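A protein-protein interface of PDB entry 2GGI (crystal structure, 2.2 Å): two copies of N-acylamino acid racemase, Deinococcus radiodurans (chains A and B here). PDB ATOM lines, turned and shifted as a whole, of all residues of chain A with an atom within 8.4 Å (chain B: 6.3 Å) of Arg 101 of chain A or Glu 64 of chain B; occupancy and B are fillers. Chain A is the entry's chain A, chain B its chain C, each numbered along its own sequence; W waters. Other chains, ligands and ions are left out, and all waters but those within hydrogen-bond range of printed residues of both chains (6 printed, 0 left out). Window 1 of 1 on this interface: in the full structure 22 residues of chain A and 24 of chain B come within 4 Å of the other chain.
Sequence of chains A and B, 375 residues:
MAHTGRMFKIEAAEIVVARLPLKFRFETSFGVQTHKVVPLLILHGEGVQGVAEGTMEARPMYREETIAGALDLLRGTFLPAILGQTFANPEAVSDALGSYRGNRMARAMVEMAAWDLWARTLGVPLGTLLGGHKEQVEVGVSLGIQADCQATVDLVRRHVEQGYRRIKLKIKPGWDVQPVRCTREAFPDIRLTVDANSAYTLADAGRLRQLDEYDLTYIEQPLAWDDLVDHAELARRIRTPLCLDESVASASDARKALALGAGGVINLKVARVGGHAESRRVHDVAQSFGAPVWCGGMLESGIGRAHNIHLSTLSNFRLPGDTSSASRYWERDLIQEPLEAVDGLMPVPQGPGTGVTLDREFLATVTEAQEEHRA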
ATOM      1  N   ARG A  63      24.966  11.380  -3.113  1.00  0.00           N
ATOM      2  CA  ARG A  63      25.092  11.216  -4.556  1.00  0.00           C
ATOM      3  C   ARG A  63      24.671  12.522  -5.234  1.00  0.00           C
ATOM      4  O   ARG A  63      24.737  13.578  -4.606  1.00  0.00           O
ATOM      5  CB  ARG A  63      24.324   9.973  -5.065  1.00  0.00           C
ATOM      6  CG  ARG A  63      25.162   9.064  -6.023  1.00  0.00           C
ATOM      7  CD  ARG A  63      24.403   7.764  -6.409  1.00  0.00           C
ATOM      8  NE  ARG A  63      25.125   6.900  -7.356  1.00  0.00           N
ATOM      9  CZ  ARG A  63      25.204   7.088  -8.683  1.00  0.00           C
ATOM     10  NH1 ARG A  63      25.889   6.223  -9.444  1.00  0.00           N
ATOM     11  NH2 ARG A  63      24.621   8.140  -9.263  1.00  0.00           N
ATOM     12  N   GLU A  64      24.233  12.466  -6.489  1.00  0.00           N
ATOM     13  CA  GLU A  64      24.177  13.666  -7.331  1.00  0.00           C
ATOM     14  C   GLU A  64      22.853  14.453  -7.328  1.00  0.00           C
ATOM     15  O   GLU A  64      22.807  15.610  -7.773  1.00  0.00           O
ATOM     16  CB  GLU A  64      24.598  13.297  -8.775  1.00  0.00           C
ATOM     17  CG  GLU A  64      23.477  12.767  -9.725  1.00  0.00           C
ATOM     18  CD  GLU A  64      23.037  11.313  -9.472  1.00  0.00           C
ATOM     19  OE1 GLU A  64      22.222  10.824 -10.272  1.00  0.00           O
ATOM     20  OE2 GLU A  64      23.466  10.659  -8.487  1.00  0.00           O
ATOM     21  N   GLU A  65      21.776  13.837  -6.847  1.00  0.00           N
ATOM     22  CA  GLU A  65      20.446  14.423  -6.986  1.00  0.00           C
ATOM     23  C   GLU A  65      20.195  15.350  -5.832  1.00  0.00           C
ATOM     24  O   GLU A  65      20.838  15.236  -4.780  1.00  0.00           O
ATOM     25  CB  GLU A  65      19.354  13.343  -7.026  1.00  0.00           C
ATOM     26  CG  GLU A  65      19.326  12.535  -8.335  1.00  0.00           C
ATOM     27  CD  GLU A  65      18.324  11.409  -8.294  1.00  0.00           C
ATOM     28  OE1 GLU A  65      17.106  11.674  -8.419  1.00  0.00           O
ATOM     29  OE2 GLU A  65      18.747  10.247  -8.104  1.00  0.00           O
ATOM     30  N   GLY A  69      15.928  19.720  -7.639  1.00  0.00           N
ATOM     31  CA  GLY A  69      15.959  19.135  -8.975  1.00  0.00           C
ATOM     32  C   GLY A  69      14.904  18.055  -9.117  1.00  0.00           C
ATOM     33  O   GLY A  69      14.155  18.003 -10.131  1.00  0.00           O
ATOM     34  N   ALA A  70      14.829  17.192  -8.100  1.00  0.00           N
ATOM     35  CA  ALA A  70      13.930  16.041  -8.148  1.00  0.00           C
ATOM     36  C   ALA A  70      12.449  16.457  -8.122  1.00  0.00           C
ATOM     37  O   ALA A  70      11.642  15.928  -8.900  1.00  0.00           O
ATOM     38  CB  ALA A  70      14.245  15.079  -7.017  1.00  0.00           C
ATOM     39  N   LEU A  73      11.419  18.016 -11.369  1.00  0.00           N
ATOM     40  CA  LEU A  73      11.271  16.945 -12.353  1.00  0.00           C
ATOM     41  C   LEU A  73       9.951  16.172 -12.180  1.00  0.00           C
ATOM     42  O   LEU A  73       9.303  15.813 -13.167  1.00  0.00           O
ATOM     43  CB  LEU A  73      12.486  16.008 -12.304  1.00  0.00           C
ATOM     44  CG  LEU A  73      12.639  14.888 -13.325  1.00  0.00           C
ATOM     45  CD1 LEU A  73      12.857  15.374 -14.761  1.00  0.00           C
ATOM     46  CD2 LEU A  73      13.800  14.018 -12.894  1.00  0.00           C
ATOM     47  N   PHE A  78       7.431  14.141 -14.669  1.00  0.00           N
ATOM     48  CA  PHE A  78       6.979  12.765 -14.427  1.00  0.00           C
ATOM     49  C   PHE A  78       5.467  12.692 -14.153  1.00  0.00           C
ATOM     50  O   PHE A  78       4.749  11.863 -14.723  1.00  0.00           O
ATOM     51  CB  PHE A  78       7.773  12.098 -13.291  1.00  0.00           C
ATOM     52  CG  PHE A  78       9.234  11.857 -13.614  1.00  0.00           C
ATOM     53  CD1 PHE A  78       9.708  11.929 -14.930  1.00  0.00           C
ATOM     54  CD2 PHE A  78      10.127  11.502 -12.599  1.00  0.00           C
ATOM     55  CE1 PHE A  78      11.062  11.681 -15.215  1.00  0.00           C
ATOM     56  CE2 PHE A  78      11.466  11.254 -12.869  1.00  0.00           C
ATOM     57  CZ  PHE A  78      11.942  11.351 -14.179  1.00  0.00           C
ATOM     58  N   LEU A  97       7.944   7.089 -18.211  1.00  0.00           N
ATOM     59  CA  LEU A  97       8.914   8.159 -17.999  1.00  0.00           C
ATOM     60  C   LEU A  97      10.007   8.017 -19.073  1.00  0.00           C
ATOM     61  O   LEU A  97       9.909   8.616 -20.153  1.00  0.00           O
ATOM     62  CB  LEU A  97       9.467   8.082 -16.574  1.00  0.00           C
ATOM     63  CG  LEU A  97       8.378   7.920 -15.502  1.00  0.00           C
ATOM     64  CD1 LEU A  97       8.952   7.899 -14.091  1.00  0.00           C
ATOM     65  CD2 LEU A  97       7.311   9.009 -15.627  1.00  0.00           C
ATOM     66  N   GLY A  98      11.041   7.230 -18.771  1.00  0.00           N
ATOM     67  CA  GLY A  98      11.830   6.528 -19.789  1.00  0.00           C
ATOM     68  C   GLY A  98      12.840   7.249 -20.664  1.00  0.00           C
ATOM     69  O   GLY A  98      13.965   6.772 -20.842  1.00  0.00           O
ATOM     70  N   SER A  99      12.449   8.371 -21.258  1.00  0.00           N
ATOM     71  CA  SER A  99      13.390   9.113 -22.103  1.00  0.00           C
ATOM     72  C   SER A  99      14.528   9.680 -21.250  1.00  0.00           C
ATOM     73  O   SER A  99      15.686   9.734 -21.675  1.00  0.00           O
ATOM     74  CB  SER A  99      12.689  10.270 -22.826  1.00  0.00           C
ATOM     75  OG  SER A  99      11.580   9.831 -23.576  1.00  0.00           O
ATOM     76  N   TYR A 100      14.180  10.083 -20.035  1.00  0.00           N
ATOM     77  CA  TYR A 100      15.031  10.949 -19.233  1.00  0.00           C
ATOM     78  C   TYR A 100      16.243  10.249 -18.632  1.00  0.00           C
ATOM     79  O   TYR A 100      16.185   9.083 -18.263  1.00  0.00           O
ATOM     80  CB  TYR A 100      14.177  11.717 -18.216  1.00  0.00           C
ATOM     81  CG  TYR A 100      13.069  12.457 -18.951  1.00  0.00           C
ATOM     82  CD1 TYR A 100      11.800  11.897 -19.093  1.00  0.00           C
ATOM     83  CD2 TYR A 100      13.318  13.684 -19.564  1.00  0.00           C
ATOM     84  CE1 TYR A 100      10.800  12.562 -19.797  1.00  0.00           C
ATOM     85  CE2 TYR A 100      12.339  14.346 -20.272  1.00  0.00           C
ATOM     86  CZ  TYR A 100      11.076  13.781 -20.387  1.00  0.00           C
ATOM     87  OH  TYR A 100      10.099  14.451 -21.097  1.00  0.00           O
ATOM     88  N   ARG A 101      17.349  10.975 -18.564  1.00  0.00           N
ATOM     89  CA  ARG A 101      18.630  10.412 -18.131  1.00  0.00           C
ATOM     90  C   ARG A 101      18.925  10.577 -16.631  1.00  0.00           C
ATOM     91  O   ARG A 101      18.683  11.644 -16.036  1.00  0.00           O
ATOM     92  CB  ARG A 101      19.761  10.974 -19.000  1.00  0.00           C
ATOM     93  CG  ARG A 101      19.613  10.541 -20.453  1.00  0.00           C
ATOM     94  CD  ARG A 101      20.834  10.799 -21.364  1.00  0.00           C
ATOM     95  NE  ARG A 101      20.672  10.030 -22.609  1.00  0.00           N
ATOM     96  CZ  ARG A 101      21.243  10.292 -23.788  1.00  0.00           C
ATOM     97  NH1 ARG A 101      22.065  11.333 -23.985  1.00  0.00           N
ATOM     98  NH2 ARG A 101      20.971   9.488 -24.801  1.00  0.00           N
ATOM     99  N   GLY A 102      19.430   9.504 -16.022  1.00  0.00           N
ATOM    100  CA  GLY A 102      19.741   9.484 -14.592  1.00  0.00           C
ATOM    101  C   GLY A 102      18.530   9.779 -13.715  1.00  0.00           C
ATOM    102  O   GLY A 102      17.432   9.274 -13.957  1.00  0.00           O
ATOM    103  N   ASN A 103      18.729  10.616 -12.702  1.00  0.00           N
ATOM    104  CA  ASN A 103      17.648  11.008 -11.810  1.00  0.00           C
ATOM    105  C   ASN A 103      16.888   9.824 -11.216  1.00  0.00           C
ATOM    106  O   ASN A 103      15.683   9.850 -11.095  1.00  0.00           O
ATOM    107  CB  ASN A 103      16.714  11.967 -12.541  1.00  0.00           C
ATOM    108  CG  ASN A 103      17.417  13.272 -12.905  1.00  0.00           C
ATOM    109  OD1 ASN A 103      17.979  13.443 -14.021  1.00  0.00           O
ATOM    110  ND2 ASN A 103      17.398  14.194 -11.966  1.00  0.00           N
ATOM    111  N   ARG A 104      17.631   8.796 -10.833  1.00  0.00           N
ATOM    112  CA  ARG A 104      17.060   7.526 -10.419  1.00  0.00           C
ATOM    113  C   ARG A 104      16.252   7.607  -9.112  1.00  0.00           C
ATOM    114  O   ARG A 104      15.221   6.936  -8.977  1.00  0.00           O
ATOM    115  CB  ARG A 104      18.156   6.445 -10.404  1.00  0.00           C
ATOM    116  CG  ARG A 104      18.374   5.843 -11.821  1.00  0.00           C
ATOM    117  CD  ARG A 104      19.616   4.985 -11.948  1.00  0.00           C
ATOM    118  NE  ARG A 104      19.728   4.372 -13.280  1.00  0.00           N
ATOM    119  CZ  ARG A 104      19.111   3.247 -13.664  1.00  0.00           C
ATOM    120  NH1 ARG A 104      18.314   2.580 -12.834  1.00  0.00           N
ATOM    121  NH2 ARG A 104      19.285   2.784 -14.900  1.00  0.00           N
ATOM    122  N   ALA A 106      14.575  10.318  -8.115  1.00  0.00           N
ATOM    123  CA  ALA A 106      13.339  10.985  -8.481  1.00  0.00           C
ATOM    124  C   ALA A 106      12.382   9.991  -9.122  1.00  0.00           C
ATOM    125  O   ALA A 106      11.192   9.951  -8.788  1.00  0.00           O
ATOM    126  CB  ALA A 106      13.603  12.152  -9.422  1.00  0.00           C
ATOM    127  N   ARG A 107      12.912   9.193 -10.044  1.00  0.00           N
ATOM    128  CA  ARG A 107      12.166   8.129 -10.698  1.00  0.00           C
ATOM    129  C   ARG A 107      11.621   7.125  -9.690  1.00  0.00           C
ATOM    130  O   ARG A 107      10.512   6.630  -9.848  1.00  0.00           O
ATOM    131  CB  ARG A 107      13.076   7.395 -11.689  1.00  0.00           C
ATOM    132  CG  ARG A 107      13.440   8.220 -12.896  1.00  0.00           C
ATOM    133  CD  ARG A 107      14.200   7.405 -13.894  1.00  0.00           C
ATOM    134  NE  ARG A 107      13.348   6.357 -14.436  1.00  0.00           N
ATOM    135  CZ  ARG A 107      12.969   6.292 -15.704  1.00  0.00           C
ATOM    136  NH1 ARG A 107      13.399   7.211 -16.564  1.00  0.00           N
ATOM    137  NH2 ARG A 107      12.174   5.303 -16.107  1.00  0.00           N
ATOM    138  N   TRP A 225      33.354   7.170  -5.328  1.00  0.00           N
ATOM    139  CA  TRP A 225      31.941   6.805  -5.214  1.00  0.00           C
ATOM    140  C   TRP A 225      31.323   6.314  -6.507  1.00  0.00           C
ATOM    141  O   TRP A 225      30.371   5.518  -6.486  1.00  0.00           O
ATOM    142  CB  TRP A 225      31.126   7.994  -4.671  1.00  0.00           C
ATOM    143  CG  TRP A 225      31.068   9.197  -5.605  1.00  0.00           C
ATOM    144  CD1 TRP A 225      31.934  10.258  -5.636  1.00  0.00           C
ATOM    145  CD2 TRP A 225      30.088   9.453  -6.627  1.00  0.00           C
ATOM    146  NE1 TRP A 225      31.556  11.144  -6.618  1.00  0.00           N
ATOM    147  CE2 TRP A 225      30.425  10.679  -7.232  1.00  0.00           C
ATOM    148  CE3 TRP A 225      28.959   8.760  -7.088  1.00  0.00           C
ATOM    149  CZ2 TRP A 225      29.681  11.228  -8.281  1.00  0.00           C
ATOM    150  CZ3 TRP A 225      28.217   9.307  -8.118  1.00  0.00           C
ATOM    151  CH2 TRP A 225      28.579  10.530  -8.703  1.00  0.00           C
ATOM    152  N   GLU B  57      19.842  21.433 -19.371  1.00  0.00           N
ATOM    153  CA  GLU B  57      18.523  21.632 -19.970  1.00  0.00           C
ATOM    154  C   GLU B  57      17.438  21.747 -18.913  1.00  0.00           C
ATOM    155  O   GLU B  57      17.629  21.362 -17.751  1.00  0.00           O
ATOM    156  CB  GLU B  57      18.176  20.443 -20.875  1.00  0.00           C
ATOM    157  CG  GLU B  57      19.250  20.060 -21.899  1.00  0.00           C
ATOM    158  CD  GLU B  57      19.262  18.564 -22.195  1.00  0.00           C
ATOM    159  OE1 GLU B  57      19.710  17.786 -21.337  1.00  0.00           O
ATOM    160  OE2 GLU B  57      18.819  18.160 -23.289  1.00  0.00           O
ATOM    161  N   PRO B  60      16.178  16.576 -18.209  1.00  0.00           N
ATOM    162  CA  PRO B  60      17.386  15.754 -18.403  1.00  0.00           C
ATOM    163  C   PRO B  60      17.298  14.807 -19.591  1.00  0.00           C
ATOM    164  O   PRO B  60      16.989  13.630 -19.432  1.00  0.00           O
ATOM    165  CB  PRO B  60      17.496  14.979 -17.085  1.00  0.00           C
ATOM    166  CG  PRO B  60      16.088  14.839 -16.621  1.00  0.00           C
ATOM    167  CD  PRO B  60      15.333  16.073 -17.110  1.00  0.00           C
ATOM    168  N   MET B  61      17.579  15.334 -20.777  1.00  0.00           N
ATOM    169  CA  MET B  61      17.421  14.584 -22.006  1.00  0.00           C
ATOM    170  C   MET B  61      18.782  14.158 -22.569  1.00  0.00           C
ATOM    171  O   MET B  61      18.983  12.990 -22.911  1.00  0.00           O
ATOM    172  CB  MET B  61      16.620  15.415 -23.024  1.00  0.00           C
ATOM    173  CG  MET B  61      15.243  15.870 -22.507  1.00  0.00           C
ATOM    174  SD  MET B  61      14.292  16.996 -23.577  1.00  0.00           S
ATOM    175  CE  MET B  61      15.413  18.381 -23.665  1.00  0.00           C
ATOM    176  N   TYR B  62      19.719  15.102 -22.646  1.00  0.00           N
ATOM    177  CA  TYR B  62      21.084  14.805 -23.076  1.00  0.00           C
ATOM    178  C   TYR B  62      21.921  14.176 -21.934  1.00  0.00           C
ATOM    179  O   TYR B  62      22.720  13.255 -22.151  1.00  0.00           O
ATOM    180  CB  TYR B  62      21.791  16.070 -23.597  1.00  0.00           C
ATOM    181  CG  TYR B  62      23.307  15.925 -23.585  1.00  0.00           C
ATOM    182  CD1 TYR B  62      24.058  16.394 -22.513  1.00  0.00           C
ATOM    183  CD2 TYR B  62      23.975  15.267 -24.621  1.00  0.00           C
ATOM    184  CE1 TYR B  62      25.437  16.242 -22.482  1.00  0.00           C
ATOM    185  CE2 TYR B  62      25.363  15.118 -24.603  1.00  0.00           C
ATOM    186  CZ  TYR B  62      26.080  15.612 -23.521  1.00  0.00           C
ATOM    187  OH  TYR B  62      27.443  15.472 -23.469  1.00  0.00           O
ATOM    188  N   ARG B  63      21.756  14.688 -20.721  1.00  0.00           N
ATOM    189  CA  ARG B  63      22.366  14.047 -19.545  1.00  0.00           C
ATOM    190  C   ARG B  63      21.520  14.343 -18.290  1.00  0.00           C
ATOM    191  O   ARG B  63      20.345  14.681 -18.408  1.00  0.00           O
ATOM    192  CB  ARG B  63      23.833  14.489 -19.373  1.00  0.00           C
ATOM    193  CG  ARG B  63      24.836  13.344 -19.183  1.00  0.00           C
ATOM    194  CD  ARG B  63      26.264  13.885 -18.952  1.00  0.00           C
ATOM    195  NE  ARG B  63      27.254  12.824 -18.760  1.00  0.00           N
ATOM    196  CZ  ARG B  63      27.546  12.270 -17.585  1.00  0.00           C
ATOM    197  NH1 ARG B  63      26.941  12.698 -16.486  1.00  0.00           N
ATOM    198  NH2 ARG B  63      28.476  11.321 -17.498  1.00  0.00           N
ATOM    199  N   GLU B  64      22.123  14.260 -17.105  1.00  0.00           N
ATOM    200  CA  GLU B  64      21.356  14.142 -15.860  1.00  0.00           C
ATOM    201  C   GLU B  64      20.990  15.473 -15.193  1.00  0.00           C
ATOM    202  O   GLU B  64      20.041  15.549 -14.411  1.00  0.00           O
ATOM    203  CB  GLU B  64      22.079  13.214 -14.866  1.00  0.00           C
ATOM    204  CG  GLU B  64      23.130  13.871 -13.937  1.00  0.00           C
ATOM    205  CD  GLU B  64      24.459  14.252 -14.616  1.00  0.00           C
ATOM    206  OE1 GLU B  64      25.398  14.649 -13.888  1.00  0.00           O
ATOM    207  OE2 GLU B  64      24.566  14.190 -15.855  1.00  0.00           O
ATOM    208  N   GLU B  65      21.731  16.527 -15.496  1.00  0.00           N
ATOM    209  CA  GLU B  65      21.475  17.805 -14.837  1.00  0.00           C
ATOM    210  C   GLU B  65      20.253  18.524 -15.426  1.00  0.00           C
ATOM    211  O   GLU B  65      19.924  18.338 -16.594  1.00  0.00           O
ATOM    212  CB  GLU B  65      22.728  18.682 -14.841  1.00  0.00           C
ATOM    213  CG  GLU B  65      23.844  18.160 -13.927  1.00  0.00           C
ATOM    214  CD  GLU B  65      25.104  19.011 -14.019  1.00  0.00           C
ATOM    215  OE1 GLU B  65      25.127  20.122 -13.437  1.00  0.00           O
ATOM    216  OE2 GLU B  65      26.081  18.578 -14.670  1.00  0.00           O
ATOM    217  N   THR B  66      19.584  19.318 -14.590  1.00  0.00           N
ATOM    218  CA  THR B  66      18.457  20.171 -14.986  1.00  0.00           C
ATOM    219  C   THR B  66      18.728  21.608 -14.553  1.00  0.00           C
ATOM    220  O   THR B  66      19.536  21.859 -13.651  1.00  0.00           O
ATOM    221  CB  THR B  66      17.138  19.723 -14.324  1.00  0.00           C
ATOM    222  OG1 THR B  66      17.205  19.929 -12.893  1.00  0.00           O
ATOM    223  CG2 THR B  66      16.869  18.232 -14.636  1.00  0.00           C
ATOM    224  N   GLY B 102      29.006  14.997  -8.414  1.00  0.00           N
ATOM    225  CA  GLY B 102      28.480  15.233  -9.743  1.00  0.00           C
ATOM    226  C   GLY B 102      28.196  16.708  -9.999  1.00  0.00           C
ATOM    227  O   GLY B 102      28.999  17.574  -9.636  1.00  0.00           O
ATOM    228  N   ASN B 103      27.052  16.979 -10.632  1.00  0.00           N
ATOM    229  CA  ASN B 103      26.659  18.340 -10.998  1.00  0.00           C
ATOM    230  C   ASN B 103      27.808  19.144 -11.612  1.00  0.00           C
ATOM    231  O   ASN B 103      28.072  20.254 -11.192  1.00  0.00           O
ATOM    232  CB  ASN B 103      26.099  19.090  -9.776  1.00  0.00           C
ATOM    233  CG  ASN B 103      24.846  18.457  -9.228  1.00  0.00           C
ATOM    234  OD1 ASN B 103      23.732  18.843  -9.597  1.00  0.00           O
ATOM    235  ND2 ASN B 103      25.014  17.473  -8.338  1.00  0.00           N
ATOM    236  N   ARG B 104      28.473  18.563 -12.602  1.00  0.00           N
ATOM    237  CA  ARG B 104      29.600  19.180 -13.311  1.00  0.00           C
ATOM    238  C   ARG B 104      29.247  20.439 -14.121  1.00  0.00           C
ATOM    239  O   ARG B 104      29.993  21.420 -14.102  1.00  0.00           O
ATOM    240  CB  ARG B 104      30.215  18.156 -14.268  1.00  0.00           C
ATOM    241  CG  ARG B 104      30.736  16.909 -13.589  1.00  0.00           C
ATOM    242  CD  ARG B 104      32.111  17.165 -13.059  1.00  0.00           C
ATOM    243  NE  ARG B 104      32.839  15.941 -12.773  1.00  0.00           N
ATOM    244  CZ  ARG B 104      34.162  15.871 -12.708  1.00  0.00           C
ATOM    245  NH1 ARG B 104      34.903  16.951 -12.943  1.00  0.00           N
ATOM    246  NH2 ARG B 104      34.749  14.719 -12.418  1.00  0.00           N
ATOM    247  N   MET B 105      28.157  20.395 -14.878  1.00  0.00           N
ATOM    248  CA  MET B 105      27.705  21.595 -15.597  1.00  0.00           C
ATOM    249  C   MET B 105      27.440  22.790 -14.675  1.00  0.00           C
ATOM    250  O   MET B 105      27.830  23.931 -14.983  1.00  0.00           O
ATOM    251  CB  MET B 105      26.503  21.275 -16.471  1.00  0.00           C
ATOM    252  CG  MET B 105      26.854  20.258 -17.562  1.00  0.00           C
ATOM    253  SD  MET B 105      25.429  19.820 -18.589  1.00  0.00           S
ATOM    254  CE  MET B 105      26.180  18.584 -19.634  1.00  0.00           C
ATOM    255  N   ASN B 197      23.991   8.333 -31.440  1.00  0.00           N
ATOM    256  CA  ASN B 197      22.924   8.771 -30.526  1.00  0.00           C
ATOM    257  C   ASN B 197      22.430   7.754 -29.506  1.00  0.00           C
ATOM    258  O   ASN B 197      21.218   7.622 -29.320  1.00  0.00           O
ATOM    259  CB  ASN B 197      21.713   9.264 -31.343  1.00  0.00           C
ATOM    260  CG  ASN B 197      20.643   9.910 -30.473  1.00  0.00           C
ATOM    261  OD1 ASN B 197      20.949  10.760 -29.632  1.00  0.00           O
ATOM    262  ND2 ASN B 197      19.384   9.508 -30.667  1.00  0.00           N
ATOM    263  N   SER B 198      23.348   7.050 -28.834  1.00  0.00           N
ATOM    264  CA  SER B 198      23.000   5.976 -27.875  1.00  0.00           C
ATOM    265  C   SER B 198      21.719   5.217 -28.202  1.00  0.00           C
ATOM    266  O   SER B 198      21.051   4.728 -27.314  1.00  0.00           O
ATOM    267  CB  SER B 198      22.914   6.504 -26.440  1.00  0.00           C
ATOM    268  OG  SER B 198      24.044   7.288 -26.125  1.00  0.00           O
ATOM    269  N   TRP B 225      24.637   6.127 -22.521  1.00  0.00           N
ATOM    270  CA  TRP B 225      25.297   7.410 -22.237  1.00  0.00           C
ATOM    271  C   TRP B 225      26.265   7.345 -21.079  1.00  0.00           C
ATOM    272  O   TRP B 225      27.183   8.167 -20.990  1.00  0.00           O
ATOM    273  CB  TRP B 225      24.264   8.507 -21.951  1.00  0.00           C
ATOM    274  CG  TRP B 225      23.479   8.247 -20.703  1.00  0.00           C
ATOM    275  CD1 TRP B 225      22.343   7.491 -20.595  1.00  0.00           C
ATOM    276  CD2 TRP B 225      23.773   8.726 -19.380  1.00  0.00           C
ATOM    277  NE1 TRP B 225      21.915   7.474 -19.285  1.00  0.00           N
ATOM    278  CE2 TRP B 225      22.776   8.216 -18.520  1.00  0.00           C
ATOM    279  CE3 TRP B 225      24.778   9.534 -18.842  1.00  0.00           C
ATOM    280  CZ2 TRP B 225      22.754   8.494 -17.149  1.00  0.00           C
ATOM    281  CZ3 TRP B 225      24.754   9.808 -17.484  1.00  0.00           C
ATOM    282  CH2 TRP B 225      23.747   9.288 -16.653  1.00  0.00           C
ATOM    283  N   GLU B 246      28.995  11.562 -23.854  1.00  0.00           N
ATOM    284  CA  GLU B 246      28.322  11.531 -22.549  1.00  0.00           C
ATOM    285  C   GLU B 246      29.064  10.784 -21.425  1.00  0.00           C
ATOM    286  O   GLU B 246      28.903  11.106 -20.243  1.00  0.00           O
ATOM    287  CB  GLU B 246      26.924  10.936 -22.696  1.00  0.00           C
ATOM    288  CG  GLU B 246      25.928  11.837 -23.410  1.00  0.00           C
ATOM    289  CD  GLU B 246      25.803  11.509 -24.897  1.00  0.00           C
ATOM    290  OE1 GLU B 246      26.836  11.210 -25.538  1.00  0.00           O
ATOM    291  OE2 GLU B 246      24.665  11.535 -25.418  1.00  0.00           O
HETATM  292  O   HOH W   1      19.583   6.387 -17.078  1.00  0.00           O
HETATM  293  O   HOH W   2      18.727   8.210 -27.122  1.00  0.00           O
HETATM  294  O   HOH W   3      17.318  11.097 -23.248  1.00  0.00           O
HETATM  295  O   HOH W   4      20.352  14.885 -11.360  1.00  0.00           O
HETATM  296  O   HOH W   5      22.460  16.329 -10.844  1.00  0.00           O
HETATM  297  O   HOH W   6      14.675  19.363 -12.412  1.00  0.00           O
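OE2 of Glu 64 of chain A is in salt-bridge range of NH2 of Arg 63 of chain A (2.9 Å). O of Leu 73 of chain A lies within hydrogen-bond range of N of Phe 78 of chain A (2.9 Å). The side-chain carboxylate (OE1) of Glu 57 of chain B is in hydrogen-bond range of the backbone NH (N) of Met 61 of chain B (3.3 Å).
Water W3 bridges O of Met 61 of chain B and O of Ser 99 of chain A. Water W5 lies within hydrogen-bond range of OD1 of Asn 103 of chain B (3.1 Å) and O of Glu 64 of chain A (3.2 Å).
The backbone carbonyl oxygen (O) of Glu 64 of chain A is in hydrogen-bond range of the side-chain amide nitrogen (ND2) of Asn 103 of chain B (2.9 Å). The backbone NH of Arg 101 of chain A is in hydrogen-bond range of the backbone carbonyl oxygen of Pro 60 of chain B (2.8 Å). NE of Arg 101 of chain A lies close to O of Met 61 of chain B, at 3.4 Å. The backbone carbonyl oxygen (O) of Tyr 62 of chain B sits at hydrogen-bond distance from the guanidinium group (NH1) of Arg 101 of chain A (2.7 Å). The side-chain carboxylate (OE2) of Glu 246 of chain B is in salt-bridge range of the guanidinium group (NH1) of Arg 101 of chain A (3.0 Å). O of Glu 64 of chain B sits close to OD1 of Asn 103 of chain A, 3.0 Å away.
Printed residues of chain B within 4 Å of Arg 101 of chain A: Pro 60 (2.8 Å), Met 61 (3.3 Å), Tyr 62 (2.7 Å), Arg 63 (3.8 Å), Glu 64 (3.7 Å), Ser 198 (3.9 Å), Trp 225 (3.6 Å) and Glu 246 (3.0 Å). Of chain A, only Arg 101 (3.7 Å) and Asn 103 (3.0 Å) come within 4 Å of Glu 64 of chain B. Of the printed residues of chain B, Leu 73 of chain A touches Pro 60 (3.5 Å). Printed residues of chain B within 4 Å of Glu 64 of chain A: Asn 103. The nearest residue of chain B that does not touch Arg 101 of chain A is Asn 197 of chain B (4.9 Å). The nearest residue of chain A that does not touch Glu 64 of chain B is Glu 64 of chain A (4.4 Å). The nearest printed residue of chain A that does not touch Met 61 of chain B is Ser 99 of chain A (4.8 Å).
Along chain A the printed residues that touch a printed residue of chain B span positions 64 to 225. Printed residues of chain B that touch a printed residue of chain A: Pro 60, Met 61, Tyr 62, Arg 63, Glu 64, Gly 102, Asn 103, Ser 198, Trp 225 and Glu 246. Hydrophobic or aromatic side chains of chain B within 4 Å of the printed part of chain A: Pro 60, Met 61 and Trp 225. Among the printed residues, Asp or Glu carboxylates within 4 Å of a Lys or Arg side-chain nitrogen of the other chain: Arg 101 of chain A with Glu 246 of chain B (3.0 Å).
Gly 102 of chain A touches Trp 225 of chain B, and with the chains exchanged Trp 225 of chain A touches Gly 102 of chain B. Of the 16 pairs that touch across the chains among the printed residues, 4 have their exchanged pair printed and touching as well.
CE2 of Tyr 100 of chain A touches CG of Met 61 of chain B, 3.97 Å away. Arg 101 of chain A touches Glu 64 of chain B (O to CA, 3.7 Å). Arg 101 of chain A touches Ser 198 of chain B. Gly 102 of chain A touches Trp 225 of chain B. OD1 of Asn 103 of chain A touches CB of Pro 60 of chain B, at 3.5 Å. Gly 102 of chain B touches Trp 225 of chain A.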
